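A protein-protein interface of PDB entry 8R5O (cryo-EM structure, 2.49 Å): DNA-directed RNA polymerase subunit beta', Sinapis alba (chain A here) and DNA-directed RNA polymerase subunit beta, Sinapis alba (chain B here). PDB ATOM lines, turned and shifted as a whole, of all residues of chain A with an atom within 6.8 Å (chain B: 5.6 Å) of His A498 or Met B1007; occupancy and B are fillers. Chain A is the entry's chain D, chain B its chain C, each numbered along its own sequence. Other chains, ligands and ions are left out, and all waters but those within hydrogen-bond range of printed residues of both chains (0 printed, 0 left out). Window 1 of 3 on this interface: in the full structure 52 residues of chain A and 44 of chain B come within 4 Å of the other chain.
The backbone carbonyl oxygen (O) of His A498 lies within hydrogen-bond range of the backbone NH (N) of Leu A451, at 2.7 Å.
Of the 9 printed residues of chain B, 4 touch a printed residue of chain A. Printed residues of chain B that touch a printed residue of chain A: Leu B995, Ile B1003, Glu B1006 and Met B1007. Hydrophobic or aromatic side chains of chain B that line the printed part of chain A: Leu B995, Ile B1003 and Met B1007. Hydrophobic or aromatic side chains of chain A that line the printed part of chain B: Leu A451, Ile A463, His A498, Leu A501 and Ala A505. Among the printed residues, 8 pairs touch across the chains.
The side-chain carboxylate of Glu B1006 is in hydrogen-bond range of the backbone NH of Leu A501, at 3.2 Å.
Among the printed residues, pairs that only touch across the chains: Leu A451 with Ile B1003 (3.6 Å), Ile A463 with Leu B995 (3.8 Å), His A498 with Glu B1006 (3.6 Å), His A498 with Met B1007 (3.6 Å), Pro A500 with Glu B1006 (3.7 Å), Ala A505 with Ile B1003 (3.4 Å) and Ala A505 with Glu B1006 (3.6 Å).
Of chain A, only His A498 (3.6 Å) comes within 4 Å of Met B1007. Of the printed residues of chain B, Pro A500 touches Glu B1006. Of the printed residues of chain B, Leu A451 touches Ile B1003 (3.6 Å). Printed residues of chain B within 4 Å of Ala A505: Ile B1003 (3.4 Å) and Glu B1006 (3.6 Å). Printed residues of chain A within 4 Å of Ile B1003: Leu A451 and Ala A505. Of the printed residues of chain B, Ile A463 touches Leu B995 (3.8 Å). The nearest residue of chain B that does not touch His A498 is Ile B1003 (4.9 Å). The nearest printed residue of chain B that does not touch Ala A505 is His B1002 (4.3 Å).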
ATOM      1  N   LEU A 405      22.666 -15.586  -9.044  1.00  0.00           N
ATOM      2  CA  LEU A 405      21.373 -16.011  -8.515  1.00  0.00           C
ATOM      3  C   LEU A 405      21.100 -15.422  -7.139  1.00  0.00           C
ATOM      4  O   LEU A 405      19.951 -15.096  -6.822  1.00  0.00           O
ATOM      5  CB  LEU A 405      21.307 -17.536  -8.450  1.00  0.00           C
ATOM      6  CG  LEU A 405      21.307 -18.294  -9.775  1.00  0.00           C
ATOM      7  CD1 LEU A 405      21.516 -19.778  -9.531  1.00  0.00           C
ATOM      8  CD2 LEU A 405      20.008 -18.049 -10.517  1.00  0.00           C
ATOM      9  N   PRO A 449      16.766 -23.258  -0.649  1.00  0.00           N
ATOM     10  CA  PRO A 449      16.672 -24.175  -1.788  1.00  0.00           C
ATOM     11  C   PRO A 449      16.434 -23.435  -3.095  1.00  0.00           C
ATOM     12  O   PRO A 449      15.950 -22.303  -3.127  1.00  0.00           O
ATOM     13  CB  PRO A 449      15.475 -25.060  -1.429  1.00  0.00           C
ATOM     14  CG  PRO A 449      14.626 -24.188  -0.576  1.00  0.00           C
ATOM     15  CD  PRO A 449      15.567 -23.309   0.203  1.00  0.00           C
ATOM     16  N   VAL A 450      16.792 -24.102  -4.193  1.00  0.00           N
ATOM     17  CA  VAL A 450      16.583 -23.584  -5.536  1.00  0.00           C
ATOM     18  C   VAL A 450      15.850 -24.636  -6.355  1.00  0.00           C
ATOM     19  O   VAL A 450      15.898 -25.832  -6.060  1.00  0.00           O
ATOM     20  CB  VAL A 450      17.906 -23.187  -6.232  1.00  0.00           C
ATOM     21  CG1 VAL A 450      18.622 -22.100  -5.443  1.00  0.00           C
ATOM     22  CG2 VAL A 450      18.801 -24.401  -6.415  1.00  0.00           C
ATOM     23  N   LEU A 451      15.158 -24.173  -7.392  1.00  0.00           N
ATOM     24  CA  LEU A 451      14.433 -25.048  -8.304  1.00  0.00           C
ATOM     25  C   LEU A 451      15.256 -25.259  -9.566  1.00  0.00           C
ATOM     26  O   LEU A 451      15.709 -24.293 -10.186  1.00  0.00           O
ATOM     27  CB  LEU A 451      13.066 -24.465  -8.664  1.00  0.00           C
ATOM     28  CG  LEU A 451      12.069 -24.185  -7.541  1.00  0.00           C
ATOM     29  CD1 LEU A 451      10.691 -23.949  -8.128  1.00  0.00           C
ATOM     30  CD2 LEU A 451      12.039 -25.316  -6.534  1.00  0.00           C
ATOM     31  N   LEU A 452      15.440 -26.519  -9.945  1.00  0.00           N
ATOM     32  CA  LEU A 452      16.186 -26.887 -11.140  1.00  0.00           C
ATOM     33  C   LEU A 452      15.239 -27.507 -12.155  1.00  0.00           C
ATOM     34  O   LEU A 452      14.486 -28.427 -11.826  1.00  0.00           O
ATOM     35  CB  LEU A 452      17.314 -27.864 -10.806  1.00  0.00           C
ATOM     36  CG  LEU A 452      18.419 -27.321  -9.900  1.00  0.00           C
ATOM     37  CD1 LEU A 452      19.512 -28.350  -9.713  1.00  0.00           C
ATOM     38  CD2 LEU A 452      18.985 -26.044 -10.476  1.00  0.00           C
ATOM     39  N   ASN A 453      15.282 -27.004 -13.382  1.00  0.00           N
ATOM     40  CA  ASN A 453      14.428 -27.520 -14.442  1.00  0.00           C
ATOM     41  C   ASN A 453      15.242 -27.890 -15.676  1.00  0.00           C
ATOM     42  O   ASN A 453      15.618 -27.026 -16.463  1.00  0.00           O
ATOM     43  CB  ASN A 453      13.355 -26.494 -14.809  1.00  0.00           C
ATOM     44  CG  ASN A 453      12.392 -27.016 -15.849  1.00  0.00           C
ATOM     45  OD1 ASN A 453      11.562 -27.877 -15.562  1.00  0.00           O
ATOM     46  ND2 ASN A 453      12.496 -26.500 -17.068  1.00  0.00           N
ATOM     47  N   ILE A 463      11.102 -30.790 -12.847  1.00  0.00           N
ATOM     48  CA  ILE A 463      11.512 -29.691 -11.981  1.00  0.00           C
ATOM     49  C   ILE A 463      11.472 -30.181 -10.540  1.00  0.00           C
ATOM     50  O   ILE A 463      10.464 -30.741 -10.094  1.00  0.00           O
ATOM     51  CB  ILE A 463      10.622 -28.450 -12.183  1.00  0.00           C
ATOM     52  CG1 ILE A 463      10.968 -27.368 -11.159  1.00  0.00           C
ATOM     53  CG2 ILE A 463       9.143 -28.816 -12.123  1.00  0.00           C
ATOM     54  CD1 ILE A 463      10.285 -26.045 -11.423  1.00  0.00           C
ATOM     55  N   ALA A 496      17.517 -24.274 -16.368  1.00  0.00           N
ATOM     56  CA  ALA A 496      16.908 -23.147 -15.680  1.00  0.00           C
ATOM     57  C   ALA A 496      17.039 -23.340 -14.177  1.00  0.00           C
ATOM     58  O   ALA A 496      16.775 -24.431 -13.663  1.00  0.00           O
ATOM     59  CB  ALA A 496      15.437 -22.994 -16.071  1.00  0.00           C
ATOM     60  N   VAL A 497      17.451 -22.285 -13.478  1.00  0.00           N
ATOM     61  CA  VAL A 497      17.546 -22.282 -12.023  1.00  0.00           C
ATOM     62  C   VAL A 497      16.700 -21.134 -11.495  1.00  0.00           C
ATOM     63  O   VAL A 497      16.870 -19.985 -11.918  1.00  0.00           O
ATOM     64  CB  VAL A 497      19.001 -22.148 -11.540  1.00  0.00           C
ATOM     65  CG1 VAL A 497      19.084 -22.397 -10.042  1.00  0.00           C
ATOM     66  CG2 VAL A 497      19.913 -23.095 -12.301  1.00  0.00           C
ATOM     67  N   HIS A 498      15.790 -21.443 -10.575  1.00  0.00           N
ATOM     68  CA  HIS A 498      14.927 -20.449  -9.952  1.00  0.00           C
ATOM     69  C   HIS A 498      15.198 -20.416  -8.456  1.00  0.00           C
ATOM     70  O   HIS A 498      15.284 -21.467  -7.814  1.00  0.00           O
ATOM     71  CB  HIS A 498      13.450 -20.750 -10.213  1.00  0.00           C
ATOM     72  CG  HIS A 498      12.512 -19.842  -9.482  1.00  0.00           C
ATOM     73  ND1 HIS A 498      12.270 -18.543  -9.878  1.00  0.00           N
ATOM     74  CD2 HIS A 498      11.763 -20.039  -8.371  1.00  0.00           C
ATOM     75  CE1 HIS A 498      11.410 -17.983  -9.047  1.00  0.00           C
ATOM     76  NE2 HIS A 498      11.087 -18.870  -8.123  1.00  0.00           N
ATOM     77  N   VAL A 499      15.334 -19.214  -7.910  1.00  0.00           N
ATOM     78  CA  VAL A 499      15.541 -19.000  -6.484  1.00  0.00           C
ATOM     79  C   VAL A 499      14.239 -18.452  -5.902  1.00  0.00           C
ATOM     80  O   VAL A 499      13.841 -17.327  -6.240  1.00  0.00           O
ATOM     81  CB  VAL A 499      16.713 -18.047  -6.217  1.00  0.00           C
ATOM     82  CG1 VAL A 499      16.867 -17.796  -4.728  1.00  0.00           C
ATOM     83  CG2 VAL A 499      18.000 -18.608  -6.800  1.00  0.00           C
ATOM     84  N   PRO A 500      13.537 -19.202  -5.053  1.00  0.00           N
ATOM     85  CA  PRO A 500      12.351 -18.646  -4.393  1.00  0.00           C
ATOM     86  C   PRO A 500      12.717 -17.437  -3.544  1.00  0.00           C
ATOM     87  O   PRO A 500      13.732 -17.429  -2.847  1.00  0.00           O
ATOM     88  CB  PRO A 500      11.848 -19.808  -3.529  1.00  0.00           C
ATOM     89  CG  PRO A 500      12.424 -21.031  -4.158  1.00  0.00           C
ATOM     90  CD  PRO A 500      13.751 -20.616  -4.709  1.00  0.00           C
ATOM     91  N   LEU A 501      11.873 -16.409  -3.607  1.00  0.00           N
ATOM     92  CA  LEU A 501      12.131 -15.157  -2.902  1.00  0.00           C
ATOM     93  C   LEU A 501      11.324 -15.050  -1.613  1.00  0.00           C
ATOM     94  O   LEU A 501      11.894 -14.880  -0.533  1.00  0.00           O
ATOM     95  CB  LEU A 501      11.835 -13.965  -3.822  1.00  0.00           C
ATOM     96  CG  LEU A 501      12.664 -13.858  -5.103  1.00  0.00           C
ATOM     97  CD1 LEU A 501      12.274 -12.621  -5.897  1.00  0.00           C
ATOM     98  CD2 LEU A 501      14.151 -13.850  -4.788  1.00  0.00           C
ATOM     99  N   ALA A 505       7.127 -19.064  -0.784  1.00  0.00           N
ATOM    100  CA  ALA A 505       7.720 -19.868  -1.846  1.00  0.00           C
ATOM    101  C   ALA A 505       8.862 -20.732  -1.330  1.00  0.00           C
ATOM    102  O   ALA A 505       9.042 -21.862  -1.799  1.00  0.00           O
ATOM    103  CB  ALA A 505       8.206 -18.965  -2.979  1.00  0.00           C
ATOM    104  N   LEU B 995       4.252 -27.913 -11.424  1.00  0.00           N
ATOM    105  CA  LEU B 995       4.070 -27.117 -10.215  1.00  0.00           C
ATOM    106  C   LEU B 995       2.655 -27.259  -9.672  1.00  0.00           C
ATOM    107  O   LEU B 995       2.454 -27.340  -8.455  1.00  0.00           O
ATOM    108  CB  LEU B 995       4.395 -25.651 -10.498  1.00  0.00           C
ATOM    109  CG  LEU B 995       5.835 -25.330 -10.898  1.00  0.00           C
ATOM    110  CD1 LEU B 995       6.009 -23.837 -11.118  1.00  0.00           C
ATOM    111  CD2 LEU B 995       6.813 -25.835  -9.852  1.00  0.00           C
ATOM    112  N   HIS B1002       2.235 -20.711  -4.437  1.00  0.00           N
ATOM    113  CA  HIS B1002       2.987 -19.466  -4.321  1.00  0.00           C
ATOM    114  C   HIS B1002       4.262 -19.478  -5.154  1.00  0.00           C
ATOM    115  O   HIS B1002       4.688 -18.423  -5.635  1.00  0.00           O
ATOM    116  CB  HIS B1002       3.309 -19.184  -2.855  1.00  0.00           C
ATOM    117  CG  HIS B1002       2.106 -18.834  -2.039  1.00  0.00           C
ATOM    118  ND1 HIS B1002       1.183 -19.773  -1.633  1.00  0.00           N
ATOM    119  CD2 HIS B1002       1.663 -17.645  -1.568  1.00  0.00           C
ATOM    120  CE1 HIS B1002       0.229 -19.180  -0.939  1.00  0.00           C
ATOM    121  NE2 HIS B1002       0.496 -17.887  -0.885  1.00  0.00           N
ATOM    122  N   ILE B1003       4.887 -20.643  -5.327  1.00  0.00           N
ATOM    123  CA  ILE B1003       6.015 -20.748  -6.247  1.00  0.00           C
ATOM    124  C   ILE B1003       5.562 -20.456  -7.671  1.00  0.00           C
ATOM    125  O   ILE B1003       6.236 -19.739  -8.421  1.00  0.00           O
ATOM    126  CB  ILE B1003       6.673 -22.135  -6.132  1.00  0.00           C
ATOM    127  CG1 ILE B1003       7.518 -22.225  -4.861  1.00  0.00           C
ATOM    128  CG2 ILE B1003       7.505 -22.442  -7.362  1.00  0.00           C
ATOM    129  CD1 ILE B1003       8.214 -23.553  -4.683  1.00  0.00           C
ATOM    130  N   LEU B1004       4.408 -20.999  -8.062  1.00  0.00           N
ATOM    131  CA  LEU B1004       3.881 -20.755  -9.400  1.00  0.00           C
ATOM    132  C   LEU B1004       3.578 -19.277  -9.615  1.00  0.00           C
ATOM    133  O   LEU B1004       3.813 -18.740 -10.702  1.00  0.00           O
ATOM    134  CB  LEU B1004       2.629 -21.603  -9.628  1.00  0.00           C
ATOM    135  CG  LEU B1004       1.971 -21.539 -11.005  1.00  0.00           C
ATOM    136  CD1 LEU B1004       2.912 -22.056 -12.081  1.00  0.00           C
ATOM    137  CD2 LEU B1004       0.671 -22.322 -11.006  1.00  0.00           C
ATOM    138  N   GLN B1005       3.049 -18.604  -8.591  1.00  0.00           N
ATOM    139  CA  GLN B1005       2.755 -17.181  -8.714  1.00  0.00           C
ATOM    140  C   GLN B1005       4.028 -16.367  -8.906  1.00  0.00           C
ATOM    141  O   GLN B1005       4.055 -15.421  -9.702  1.00  0.00           O
ATOM    142  CB  GLN B1005       1.985 -16.696  -7.486  1.00  0.00           C
ATOM    143  CG  GLN B1005       1.401 -15.302  -7.627  1.00  0.00           C
ATOM    144  CD  GLN B1005       0.701 -14.838  -6.367  1.00  0.00           C
ATOM    145  OE1 GLN B1005       0.934 -15.369  -5.282  1.00  0.00           O
ATOM    146  NE2 GLN B1005      -0.165 -13.841  -6.505  1.00  0.00           N
ATOM    147  N   GLU B1006       5.094 -16.715  -8.179  1.00  0.00           N
ATOM    148  CA  GLU B1006       6.366 -16.012  -8.339  1.00  0.00           C
ATOM    149  C   GLU B1006       6.932 -16.192  -9.740  1.00  0.00           C
ATOM    150  O   GLU B1006       7.423 -15.234 -10.348  1.00  0.00           O
ATOM    151  CB  GLU B1006       7.375 -16.501  -7.302  1.00  0.00           C
ATOM    152  CG  GLU B1006       7.338 -15.772  -5.976  1.00  0.00           C
ATOM    153  CD  GLU B1006       8.569 -16.050  -5.137  1.00  0.00           C
ATOM    154  OE1 GLU B1006       9.479 -16.748  -5.631  1.00  0.00           O
ATOM    155  OE2 GLU B1006       8.630 -15.569  -3.987  1.00  0.00           O
ATOM    156  N   MET B1007       6.876 -17.413 -10.273  1.00  0.00           N
ATOM    157  CA  MET B1007       7.464 -17.696 -11.574  1.00  0.00           C
ATOM    158  C   MET B1007       6.631 -17.170 -12.734  1.00  0.00           C
ATOM    159  O   MET B1007       7.091 -17.225 -13.878  1.00  0.00           O
ATOM    160  CB  MET B1007       7.683 -19.202 -11.732  1.00  0.00           C
ATOM    161  CG  MET B1007       8.775 -19.753 -10.829  1.00  0.00           C
ATOM    162  SD  MET B1007       9.046 -21.523 -11.028  1.00  0.00           S
ATOM    163  CE  MET B1007       9.404 -21.619 -12.778  1.00  0.00           C
ATOM    164  N   LEU B1008       5.426 -16.668 -12.471  1.00  0.00           N
ATOM    165  CA  LEU B1008       4.616 -16.024 -13.495  1.00  0.00           C
ATOM    166  C   LEU B1008       4.666 -14.507 -13.425  1.00  0.00           C
ATOM    167  O   LEU B1008       4.483 -13.846 -14.452  1.00  0.00           O
ATOM    168  CB  LEU B1008       3.156 -16.477 -13.380  1.00  0.00           C
ATOM    169  CG  LEU B1008       2.844 -17.941 -13.684  1.00  0.00           C
ATOM    170  CD1 LEU B1008       1.384 -18.243 -13.398  1.00  0.00           C
ATOM    171  CD2 LEU B1008       3.188 -18.276 -15.124  1.00  0.00           C
ATOM    172  N   THR B1009       4.908 -13.943 -12.247  1.00  0.00           N
ATOM    173  CA  THR B1009       4.923 -12.498 -12.076  1.00  0.00           C
ATOM    174  C   THR B1009       6.328 -12.000 -11.755  1.00  0.00           C
ATOM    175  O   THR B1009       6.523 -10.824 -11.447  1.00  0.00           O
ATOM    176  CB  THR B1009       3.964 -12.053 -10.958  1.00  0.00           C
ATOM    177  OG1 THR B1009       4.449 -12.517  -9.693  1.00  0.00           O
ATOM    178  CG2 THR B1009       2.571 -12.620 -11.194  1.00  0.00           C
